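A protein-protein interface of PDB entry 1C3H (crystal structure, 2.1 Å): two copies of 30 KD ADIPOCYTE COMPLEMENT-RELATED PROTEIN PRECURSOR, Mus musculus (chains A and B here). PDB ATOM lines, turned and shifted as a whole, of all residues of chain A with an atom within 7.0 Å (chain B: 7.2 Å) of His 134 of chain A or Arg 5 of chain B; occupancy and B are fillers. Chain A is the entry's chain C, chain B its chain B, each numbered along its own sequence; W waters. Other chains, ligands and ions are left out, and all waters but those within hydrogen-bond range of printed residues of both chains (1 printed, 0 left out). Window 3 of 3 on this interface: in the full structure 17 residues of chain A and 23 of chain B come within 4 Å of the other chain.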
ATOM      1  N   TYR A   2      14.345  -4.555  -6.303  1.00  0.00           N
ATOM      2  CA  TYR A   2      13.872  -3.177  -6.171  1.00  0.00           C
ATOM      3  C   TYR A   2      13.249  -2.531  -7.405  1.00  0.00           C
ATOM      4  O   TYR A   2      13.694  -2.740  -8.534  1.00  0.00           O
ATOM      5  CB  TYR A   2      15.012  -2.272  -5.694  1.00  0.00           C
ATOM      6  CG  TYR A   2      14.592  -0.825  -5.544  1.00  0.00           C
ATOM      7  CD1 TYR A   2      13.835  -0.408  -4.450  1.00  0.00           C
ATOM      8  CD2 TYR A   2      14.919   0.120  -6.516  1.00  0.00           C
ATOM      9  CE1 TYR A   2      13.413   0.912  -4.325  1.00  0.00           C
ATOM     10  CE2 TYR A   2      14.501   1.443  -6.401  1.00  0.00           C
ATOM     11  CZ  TYR A   2      13.749   1.832  -5.304  1.00  0.00           C
ATOM     12  OH  TYR A   2      13.334   3.139  -5.186  1.00  0.00           O
ATOM     13  N   TYR A   4      11.618   1.398  -8.632  1.00  0.00           N
ATOM     14  CA  TYR A   4      11.475   2.800  -8.282  1.00  0.00           C
ATOM     15  C   TYR A   4       9.994   3.134  -8.137  1.00  0.00           C
ATOM     16  O   TYR A   4       9.294   3.366  -9.120  1.00  0.00           O
ATOM     17  CB  TYR A   4      12.144   3.672  -9.344  1.00  0.00           C
ATOM     18  CG  TYR A   4      13.658   3.695  -9.228  1.00  0.00           C
ATOM     19  CD1 TYR A   4      14.295   4.506  -8.284  1.00  0.00           C
ATOM     20  CD2 TYR A   4      14.453   2.884 -10.043  1.00  0.00           C
ATOM     21  CE1 TYR A   4      15.690   4.515  -8.152  1.00  0.00           C
ATOM     22  CE2 TYR A   4      15.846   2.880  -9.921  1.00  0.00           C
ATOM     23  CZ  TYR A   4      16.459   3.701  -8.972  1.00  0.00           C
ATOM     24  OH  TYR A   4      17.837   3.706  -8.859  1.00  0.00           O
ATOM     25  N   ILE A  47      12.871  10.218  -5.544  1.00  0.00           N
ATOM     26  CA  ILE A  47      13.120   9.587  -6.838  1.00  0.00           C
ATOM     27  C   ILE A  47      12.810  10.587  -7.938  1.00  0.00           C
ATOM     28  O   ILE A  47      11.685  11.081  -8.042  1.00  0.00           O
ATOM     29  CB  ILE A  47      12.220   8.352  -7.049  1.00  0.00           C
ATOM     30  CG1 ILE A  47      12.464   7.332  -5.937  1.00  0.00           C
ATOM     31  CG2 ILE A  47      12.480   7.751  -8.433  1.00  0.00           C
ATOM     32  CD1 ILE A  47      11.507   6.158  -5.955  1.00  0.00           C
ATOM     33  N   PRO A  48      13.805  10.895  -8.785  1.00  0.00           N
ATOM     34  CA  PRO A  48      13.591  11.851  -9.870  1.00  0.00           C
ATOM     35  C   PRO A  48      12.696  11.276 -10.963  1.00  0.00           C
ATOM     36  O   PRO A  48      12.851  10.120 -11.376  1.00  0.00           O
ATOM     37  CB  PRO A  48      15.014  12.142 -10.355  1.00  0.00           C
ATOM     38  CG  PRO A  48      15.689  10.833 -10.176  1.00  0.00           C
ATOM     39  CD  PRO A  48      15.172  10.342  -8.830  1.00  0.00           C
ATOM     40  N   GLY A  49      11.752  12.089 -11.420  1.00  0.00           N
ATOM     41  CA  GLY A  49      10.848  11.632 -12.456  1.00  0.00           C
ATOM     42  C   GLY A  49       9.589  12.467 -12.537  1.00  0.00           C
ATOM     43  O   GLY A  49       9.497  13.543 -11.934  1.00  0.00           O
ATOM     44  N   LEU A  50       8.613  11.953 -13.279  1.00  0.00           N
ATOM     45  CA  LEU A  50       7.340  12.625 -13.479  1.00  0.00           C
ATOM     46  C   LEU A  50       6.318  12.110 -12.478  1.00  0.00           C
ATOM     47  O   LEU A  50       6.042  10.907 -12.405  1.00  0.00           O
ATOM     48  CB  LEU A  50       6.834  12.357 -14.895  1.00  0.00           C
ATOM     49  CG  LEU A  50       6.036  13.404 -15.674  1.00  0.00           C
ATOM     50  CD1 LEU A  50       4.986  12.667 -16.481  1.00  0.00           C
ATOM     51  CD2 LEU A  50       5.405  14.442 -14.772  1.00  0.00           C
ATOM     52  N   HIS A  97       7.491  17.392 -12.898  1.00  0.00           N
ATOM     53  CA  HIS A  97       8.729  16.640 -12.926  1.00  0.00           C
ATOM     54  C   HIS A  97       9.435  17.101 -11.668  1.00  0.00           C
ATOM     55  O   HIS A  97       9.500  18.301 -11.390  1.00  0.00           O
ATOM     56  CB  HIS A  97       9.580  16.973 -14.150  1.00  0.00           C
ATOM     57  CG  HIS A  97      10.906  16.288 -14.137  1.00  0.00           C
ATOM     58  ND1 HIS A  97      11.968  16.746 -13.390  1.00  0.00           N
ATOM     59  CD2 HIS A  97      11.308  15.117 -14.686  1.00  0.00           C
ATOM     60  CE1 HIS A  97      12.967  15.886 -13.476  1.00  0.00           C
ATOM     61  NE2 HIS A  97      12.593  14.889 -14.256  1.00  0.00           N
ATOM     62  N   LEU A 131       4.626   8.469  -8.452  1.00  0.00           N
ATOM     63  CA  LEU A 131       5.622   8.548  -9.493  1.00  0.00           C
ATOM     64  C   LEU A 131       5.044   7.850 -10.719  1.00  0.00           C
ATOM     65  O   LEU A 131       4.576   6.712 -10.633  1.00  0.00           O
ATOM     66  CB  LEU A 131       6.896   7.838  -9.039  1.00  0.00           C
ATOM     67  CG  LEU A 131       7.959   7.630 -10.117  1.00  0.00           C
ATOM     68  CD1 LEU A 131       8.384   8.984 -10.676  1.00  0.00           C
ATOM     69  CD2 LEU A 131       9.147   6.886  -9.515  1.00  0.00           C
ATOM     70  N   LEU A 132       5.064   8.540 -11.847  1.00  0.00           N
ATOM     71  CA  LEU A 132       4.561   7.996 -13.094  1.00  0.00           C
ATOM     72  C   LEU A 132       5.758   7.397 -13.836  1.00  0.00           C
ATOM     73  O   LEU A 132       5.802   6.190 -14.101  1.00  0.00           O
ATOM     74  CB  LEU A 132       3.955   9.118 -13.941  1.00  0.00           C
ATOM     75  CG  LEU A 132       2.712   8.864 -14.793  1.00  0.00           C
ATOM     76  CD1 LEU A 132       2.653   9.941 -15.873  1.00  0.00           C
ATOM     77  CD2 LEU A 132       2.740   7.483 -15.431  1.00  0.00           C
ATOM     78  N   TYR A 133       6.728   8.259 -14.144  1.00  0.00           N
ATOM     79  CA  TYR A 133       7.935   7.877 -14.874  1.00  0.00           C
ATOM     80  C   TYR A 133       9.240   8.244 -14.166  1.00  0.00           C
ATOM     81  O   TYR A 133       9.448   9.399 -13.815  1.00  0.00           O
ATOM     82  CB  TYR A 133       7.972   8.553 -16.252  1.00  0.00           C
ATOM     83  CG  TYR A 133       6.776   8.325 -17.144  1.00  0.00           C
ATOM     84  CD1 TYR A 133       6.249   7.050 -17.336  1.00  0.00           C
ATOM     85  CD2 TYR A 133       6.205   9.388 -17.843  1.00  0.00           C
ATOM     86  CE1 TYR A 133       5.182   6.842 -18.205  1.00  0.00           C
ATOM     87  CE2 TYR A 133       5.145   9.196 -18.717  1.00  0.00           C
ATOM     88  CZ  TYR A 133       4.636   7.925 -18.896  1.00  0.00           C
ATOM     89  OH  TYR A 133       3.591   7.736 -19.773  1.00  0.00           O
ATOM     90  N   HIS A 134      10.122   7.261 -13.992  1.00  0.00           N
ATOM     91  CA  HIS A 134      11.431   7.477 -13.370  1.00  0.00           C
ATOM     92  C   HIS A 134      12.344   8.089 -14.430  1.00  0.00           C
ATOM     93  O   HIS A 134      12.285   7.695 -15.586  1.00  0.00           O
ATOM     94  CB  HIS A 134      12.034   6.147 -12.910  1.00  0.00           C
ATOM     95  CG  HIS A 134      13.384   6.285 -12.272  1.00  0.00           C
ATOM     96  ND1 HIS A 134      14.301   5.254 -12.231  1.00  0.00           N
ATOM     97  CD2 HIS A 134      13.955   7.323 -11.614  1.00  0.00           C
ATOM     98  CE1 HIS A 134      15.377   5.653 -11.577  1.00  0.00           C
ATOM     99  NE2 HIS A 134      15.194   6.904 -11.191  1.00  0.00           N
ATOM    100  N   ASP A 135      13.193   9.037 -14.039  1.00  0.00           N
ATOM    101  CA  ASP A 135      14.104   9.696 -14.979  1.00  0.00           C
ATOM    102  C   ASP A 135      15.214   8.853 -15.613  1.00  0.00           C
ATOM    103  O   ASP A 135      15.708   7.892 -15.028  1.00  0.00           O
ATOM    104  CB  ASP A 135      14.762  10.908 -14.326  1.00  0.00           C
ATOM    105  CG  ASP A 135      13.906  12.144 -14.398  1.00  0.00           C
ATOM    106  OD1 ASP A 135      12.925  12.148 -15.173  1.00  0.00           O
ATOM    107  OD2 ASP A 135      14.227  13.118 -13.685  1.00  0.00           O
ATOM    108  N   THR A 136      15.600   9.276 -16.818  1.00  0.00           N
ATOM    109  CA  THR A 136      16.649   8.678 -17.648  1.00  0.00           C
ATOM    110  C   THR A 136      17.144   7.281 -17.273  1.00  0.00           C
ATOM    111  O   THR A 136      16.392   6.304 -17.338  1.00  0.00           O
ATOM    112  CB  THR A 136      17.886   9.618 -17.723  1.00  0.00           C
ATOM    113  OG1 THR A 136      17.453  10.962 -17.968  1.00  0.00           O
ATOM    114  CG2 THR A 136      18.825   9.191 -18.855  1.00  0.00           C
ATOM    115  N   ASN A 137      18.424   7.213 -16.900  1.00  0.00           N
ATOM    116  CA  ASN A 137      19.126   5.985 -16.520  1.00  0.00           C
ATOM    117  C   ASN A 137      19.749   5.312 -17.737  1.00  0.00           C
ATOM    118  O   ASN A 137      20.995   5.229 -17.775  1.00  0.00           O
ATOM    119  CB  ASN A 137      18.191   4.999 -15.815  1.00  0.00           C
ATOM    120  CG  ASN A 137      17.950   5.360 -14.365  1.00  0.00           C
ATOM    121  OD1 ASN A 137      18.858   5.292 -13.536  1.00  0.00           O
ATOM    122  ND2 ASN A 137      16.723   5.755 -14.051  1.00  0.00           N
ATOM    123  OXT ASN A 137      18.990   4.882 -18.636  1.00  0.00           O
ATOM    124  N   TYR B   2      15.184   3.288 -24.941  1.00  0.00           N
ATOM    125  CA  TYR B   2      13.860   3.874 -25.124  1.00  0.00           C
ATOM    126  C   TYR B   2      12.746   3.204 -24.325  1.00  0.00           C
ATOM    127  O   TYR B   2      12.732   1.988 -24.136  1.00  0.00           O
ATOM    128  CB  TYR B   2      13.467   3.860 -26.604  1.00  0.00           C
ATOM    129  CG  TYR B   2      12.089   4.430 -26.862  1.00  0.00           C
ATOM    130  CD1 TYR B   2      11.856   5.806 -26.799  1.00  0.00           C
ATOM    131  CD2 TYR B   2      11.010   3.592 -27.138  1.00  0.00           C
ATOM    132  CE1 TYR B   2      10.577   6.332 -27.003  1.00  0.00           C
ATOM    133  CE2 TYR B   2       9.731   4.108 -27.344  1.00  0.00           C
ATOM    134  CZ  TYR B   2       9.520   5.476 -27.276  1.00  0.00           C
ATOM    135  OH  TYR B   2       8.254   5.981 -27.477  1.00  0.00           O
ATOM    136  N   MET B   3      11.804   4.025 -23.877  1.00  0.00           N
ATOM    137  CA  MET B   3      10.654   3.564 -23.115  1.00  0.00           C
ATOM    138  C   MET B   3       9.430   4.297 -23.642  1.00  0.00           C
ATOM    139  O   MET B   3       9.469   5.509 -23.864  1.00  0.00           O
ATOM    140  CB  MET B   3      10.854   3.861 -21.629  1.00  0.00           C
ATOM    141  CG  MET B   3      11.933   3.007 -20.990  1.00  0.00           C
ATOM    142  SD  MET B   3      12.539   3.691 -19.445  1.00  0.00           S
ATOM    143  CE  MET B   3      13.958   4.620 -20.038  1.00  0.00           C
ATOM    144  N   TYR B   4       8.349   3.558 -23.859  1.00  0.00           N
ATOM    145  CA  TYR B   4       7.126   4.150 -24.374  1.00  0.00           C
ATOM    146  C   TYR B   4       6.508   5.069 -23.327  1.00  0.00           C
ATOM    147  O   TYR B   4       5.799   4.634 -22.416  1.00  0.00           O
ATOM    148  CB  TYR B   4       6.168   3.040 -24.815  1.00  0.00           C
ATOM    149  CG  TYR B   4       6.590   2.410 -26.132  1.00  0.00           C
ATOM    150  CD1 TYR B   4       6.340   3.056 -27.346  1.00  0.00           C
ATOM    151  CD2 TYR B   4       7.286   1.195 -26.165  1.00  0.00           C
ATOM    152  CE1 TYR B   4       6.768   2.515 -28.560  1.00  0.00           C
ATOM    153  CE2 TYR B   4       7.725   0.642 -27.376  1.00  0.00           C
ATOM    154  CZ  TYR B   4       7.460   1.311 -28.572  1.00  0.00           C
ATOM    155  OH  TYR B   4       7.872   0.777 -29.776  1.00  0.00           O
ATOM    156  N   ARG B   5       6.811   6.353 -23.466  1.00  0.00           N
ATOM    157  CA  ARG B   5       6.337   7.373 -22.544  1.00  0.00           C
ATOM    158  C   ARG B   5       5.647   8.511 -23.258  1.00  0.00           C
ATOM    159  O   ARG B   5       6.087   8.966 -24.307  1.00  0.00           O
ATOM    160  CB  ARG B   5       7.512   7.908 -21.730  1.00  0.00           C
ATOM    161  CG  ARG B   5       8.105   6.848 -20.828  1.00  0.00           C
ATOM    162  CD  ARG B   5       9.299   7.357 -20.067  1.00  0.00           C
ATOM    163  NE  ARG B   5       9.552   6.534 -18.890  1.00  0.00           N
ATOM    164  CZ  ARG B   5      10.519   6.773 -18.012  1.00  0.00           C
ATOM    165  NH1 ARG B   5      11.327   7.809 -18.186  1.00  0.00           N
ATOM    166  NH2 ARG B   5      10.665   5.984 -16.955  1.00  0.00           N
ATOM    167  N   SER B   6       4.546   8.967 -22.678  1.00  0.00           N
ATOM    168  CA  SER B   6       3.789  10.050 -23.260  1.00  0.00           C
ATOM    169  C   SER B   6       2.908  10.665 -22.194  1.00  0.00           C
ATOM    170  O   SER B   6       2.036  10.000 -21.634  1.00  0.00           O
ATOM    171  CB  SER B   6       2.927   9.532 -24.411  1.00  0.00           C
ATOM    172  OG  SER B   6       2.068  10.561 -24.866  1.00  0.00           O
ATOM    173  N   ALA B   7       3.125  11.944 -21.924  1.00  0.00           N
ATOM    174  CA  ALA B   7       2.346  12.623 -20.911  1.00  0.00           C
ATOM    175  C   ALA B   7       2.415  14.121 -21.120  1.00  0.00           C
ATOM    176  O   ALA B   7       3.362  14.637 -21.721  1.00  0.00           O
ATOM    177  CB  ALA B   7       2.880  12.273 -19.534  1.00  0.00           C
ATOM    178  N   TYR B  30       4.126  20.370 -18.075  1.00  0.00           N
ATOM    179  CA  TYR B  30       4.903  19.259 -18.598  1.00  0.00           C
ATOM    180  C   TYR B  30       4.443  18.902 -19.998  1.00  0.00           C
ATOM    181  O   TYR B  30       3.246  18.805 -20.255  1.00  0.00           O
ATOM    182  CB  TYR B  30       4.770  18.034 -17.697  1.00  0.00           C
ATOM    183  CG  TYR B  30       5.610  16.870 -18.163  1.00  0.00           C
ATOM    184  CD1 TYR B  30       6.929  16.714 -17.733  1.00  0.00           C
ATOM    185  CD2 TYR B  30       5.090  15.930 -19.052  1.00  0.00           C
ATOM    186  CE1 TYR B  30       7.708  15.639 -18.175  1.00  0.00           C
ATOM    187  CE2 TYR B  30       5.853  14.862 -19.503  1.00  0.00           C
ATOM    188  CZ  TYR B  30       7.156  14.717 -19.061  1.00  0.00           C
ATOM    189  OH  TYR B  30       7.884  13.633 -19.497  1.00  0.00           O
ATOM    190  N   GLN B  32       7.190  17.137 -22.213  1.00  0.00           N
ATOM    191  CA  GLN B  32       8.475  16.643 -22.683  1.00  0.00           C
ATOM    192  C   GLN B  32       8.498  15.942 -24.038  1.00  0.00           C
ATOM    193  O   GLN B  32       9.417  16.164 -24.825  1.00  0.00           O
ATOM    194  CB  GLN B  32       9.099  15.735 -21.619  1.00  0.00           C
ATOM    195  CG  GLN B  32      10.583  15.474 -21.829  1.00  0.00           C
ATOM    196  CD  GLN B  32      11.239  14.811 -20.631  1.00  0.00           C
ATOM    197  OE1 GLN B  32      11.214  15.345 -19.516  1.00  0.00           O
ATOM    198  NE2 GLN B  32      11.837  13.644 -20.853  1.00  0.00           N
ATOM    199  N   GLN B  33       7.508  15.100 -24.322  1.00  0.00           N
ATOM    200  CA  GLN B  33       7.483  14.404 -25.606  1.00  0.00           C
ATOM    201  C   GLN B  33       6.842  15.274 -26.672  1.00  0.00           C
ATOM    202  O   GLN B  33       6.761  14.890 -27.837  1.00  0.00           O
ATOM    203  CB  GLN B  33       6.718  13.076 -25.505  1.00  0.00           C
ATOM    204  CG  GLN B  33       7.292  12.095 -24.497  1.00  0.00           C
ATOM    205  CD  GLN B  33       6.912  12.432 -23.075  1.00  0.00           C
ATOM    206  OE1 GLN B  33       7.648  12.128 -22.130  1.00  0.00           O
ATOM    207  NE2 GLN B  33       5.752  13.052 -22.910  1.00  0.00           N
ATOM    208  N   HIS B  35       3.850  15.844 -27.260  1.00  0.00           N
ATOM    209  CA  HIS B  35       2.702  15.216 -27.887  1.00  0.00           C
ATOM    210  C   HIS B  35       1.502  16.144 -27.796  1.00  0.00           C
ATOM    211  O   HIS B  35       0.510  15.962 -28.493  1.00  0.00           O
ATOM    212  CB  HIS B  35       2.397  13.872 -27.233  1.00  0.00           C
ATOM    213  CG  HIS B  35       3.471  12.852 -27.439  1.00  0.00           C
ATOM    214  ND1 HIS B  35       4.279  12.842 -28.556  1.00  0.00           N
ATOM    215  CD2 HIS B  35       3.855  11.800 -26.686  1.00  0.00           C
ATOM    216  CE1 HIS B  35       5.117  11.823 -28.480  1.00  0.00           C
ATOM    217  NE2 HIS B  35       4.880  11.176 -27.354  1.00  0.00           N
ATOM    218  N   ASN B  46       0.826   9.300 -29.972  1.00  0.00           N
ATOM    219  CA  ASN B  46       1.947   8.839 -30.782  1.00  0.00           C
ATOM    220  C   ASN B  46       2.344   7.439 -30.348  1.00  0.00           C
ATOM    221  O   ASN B  46       3.283   6.856 -30.885  1.00  0.00           O
ATOM    222  CB  ASN B  46       3.151   9.774 -30.631  1.00  0.00           C
ATOM    223  CG  ASN B  46       3.006  11.050 -31.437  1.00  0.00           C
ATOM    224  OD1 ASN B  46       2.150  11.894 -31.150  1.00  0.00           O
ATOM    225  ND2 ASN B  46       3.838  11.194 -32.459  1.00  0.00           N
ATOM    226  N   ILE B  47       1.623   6.916 -29.361  1.00  0.00           N
ATOM    227  CA  ILE B  47       1.879   5.587 -28.826  1.00  0.00           C
ATOM    228  C   ILE B  47       0.520   4.965 -28.496  1.00  0.00           C
ATOM    229  O   ILE B  47      -0.235   5.507 -27.690  1.00  0.00           O
ATOM    230  CB  ILE B  47       2.719   5.667 -27.538  1.00  0.00           C
ATOM    231  CG1 ILE B  47       4.013   6.442 -27.804  1.00  0.00           C
ATOM    232  CG2 ILE B  47       3.017   4.273 -27.027  1.00  0.00           C
ATOM    233  CD1 ILE B  47       4.840   6.694 -26.571  1.00  0.00           C
ATOM    234  N   TYR B  51      -4.791   5.567 -21.974  1.00  0.00           N
ATOM    235  CA  TYR B  51      -4.416   6.869 -21.434  1.00  0.00           C
ATOM    236  C   TYR B  51      -5.397   7.346 -20.375  1.00  0.00           C
ATOM    237  O   TYR B  51      -6.602   7.094 -20.467  1.00  0.00           O
ATOM    238  CB  TYR B  51      -4.388   7.936 -22.532  1.00  0.00           C
ATOM    239  CG  TYR B  51      -3.237   7.822 -23.498  1.00  0.00           C
ATOM    240  CD1 TYR B  51      -3.185   6.787 -24.432  1.00  0.00           C
ATOM    241  CD2 TYR B  51      -2.170   8.721 -23.446  1.00  0.00           C
ATOM    242  CE1 TYR B  51      -2.093   6.645 -25.287  1.00  0.00           C
ATOM    243  CE2 TYR B  51      -1.071   8.584 -24.295  1.00  0.00           C
ATOM    244  CZ  TYR B  51      -1.042   7.539 -25.212  1.00  0.00           C
ATOM    245  OH  TYR B  51       0.049   7.369 -26.033  1.00  0.00           O
ATOM    246  N   LEU B 131       0.071   8.222 -20.682  1.00  0.00           N
ATOM    247  CA  LEU B 131      -0.039   6.852 -21.130  1.00  0.00           C
ATOM    248  C   LEU B 131       0.115   5.969 -19.907  1.00  0.00           C
ATOM    249  O   LEU B 131       1.107   6.061 -19.185  1.00  0.00           O
ATOM    250  CB  LEU B 131       1.076   6.541 -22.130  1.00  0.00           C
ATOM    251  CG  LEU B 131       1.252   5.064 -22.489  1.00  0.00           C
ATOM    252  CD1 LEU B 131      -0.029   4.524 -23.115  1.00  0.00           C
ATOM    253  CD2 LEU B 131       2.425   4.925 -23.444  1.00  0.00           C
ATOM    254  N   HIS B 134       0.991   0.700 -22.549  1.00  0.00           N
ATOM    255  CA  HIS B 134       1.299   0.646 -23.981  1.00  0.00           C
ATOM    256  C   HIS B 134       0.628  -0.603 -24.540  1.00  0.00           C
ATOM    257  O   HIS B 134       0.631  -1.639 -23.894  1.00  0.00           O
ATOM    258  CB  HIS B 134       2.807   0.523 -24.214  1.00  0.00           C
ATOM    259  CG  HIS B 134       3.185   0.426 -25.662  1.00  0.00           C
ATOM    260  ND1 HIS B 134       4.384  -0.108 -26.088  1.00  0.00           N
ATOM    261  CD2 HIS B 134       2.535   0.828 -26.782  1.00  0.00           C
ATOM    262  CE1 HIS B 134       4.455  -0.031 -27.406  1.00  0.00           C
ATOM    263  NE2 HIS B 134       3.346   0.532 -27.851  1.00  0.00           N
HETATM  264  O   HOH W   1       9.024   4.657 -14.387  1.00  0.00           O
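Positions printed for both chains: 2, 4, 47, 131 and 134.
O of His 134 of chain A lies within hydrogen-bond range of NH2 of Arg 5 of chain B.
The backbone NH (N) of Ser 6 of chain B sits at hydrogen-bond distance from the side-chain hydroxyl (OH) of Tyr 133 of chain A.
The side-chain hydroxyl (OH) of Tyr 133 of chain A lies within hydrogen-bond range of the backbone carbonyl oxygen (O) of Leu 131 of chain B (3.1 Å).
His 134 of chain A touches one residue of chain B.
Of chain A, only Tyr 133 (3.6 Å) and His 134 (2.7 Å) come within 4 Å of Arg 5 of chain B.
Of the printed residues of chain A, Tyr 30 of chain B touches Leu 50.
Of the printed residues of chain B, Tyr 133 of chain A touches Arg 5 (3.6 Å), Ser 6 (3.3 Å), Ala 7 (3.9 Å) and Leu 131 (3.1 Å).
The nearest residue of chain B that does not touch His 134 of chain A is Met 3 of chain B (5.6 Å).
The nearest residue of chain A that does not touch Arg 5 of chain B is Asp 135 of chain A (4.6 Å).
The nearest printed residue of chain A that does not touch Tyr 30 of chain B is His 97 of chain A (4.5 Å).
The backbone carbonyl oxygen (O) of Ser 6 of chain B is in hydrogen-bond range of the backbone NH (N) of Leu 131 of chain B.
N of Ala 7 of chain B sits close to NE2 of Gln 33 of chain B, 3.0 Å away.
The side-chain amide oxygen (OE1) of Gln 33 of chain B lies within hydrogen-bond range of the side-chain hydroxyl (OH) of Tyr 30 of chain B (3.0 Å).
The backbone carbonyl oxygen (O) of Leu 50 of chain A sits at hydrogen-bond distance from the backbone NH (N) of Leu 132 of chain A (2.6 Å).
The backbone NH (N) of Leu 50 of chain A lies within hydrogen-bond range of the backbone carbonyl oxygen (O) of Tyr 133 of chain A (2.7 Å).
A ring nitrogen (ND1) of His 134 of chain A lies close to the side-chain amide nitrogen (ND2) of Asn 137 of chain A (3.1 Å).
Among the printed residues, pairs that only touch across the chains: Tyr 133 of chain A with Arg 5 of chain B (3.6 Å), Leu 50 of chain A with Ala 7 of chain B (3.7 Å), Leu 50 of chain A with Tyr 30 of chain B (3.7 Å) and Tyr 133 of chain A with Ala 7 of chain B (3.9 Å).
Of the 15 printed residues of chain B, 5 touch a printed residue of chain A.
Along chain A the printed residues that touch a printed residue of chain B span positions 50 to 134.
Water W1 lies within hydrogen-bond range of N of His 134 of chain A (2.9 Å) and NH2 of Arg 5 of chain B (3.3 Å).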
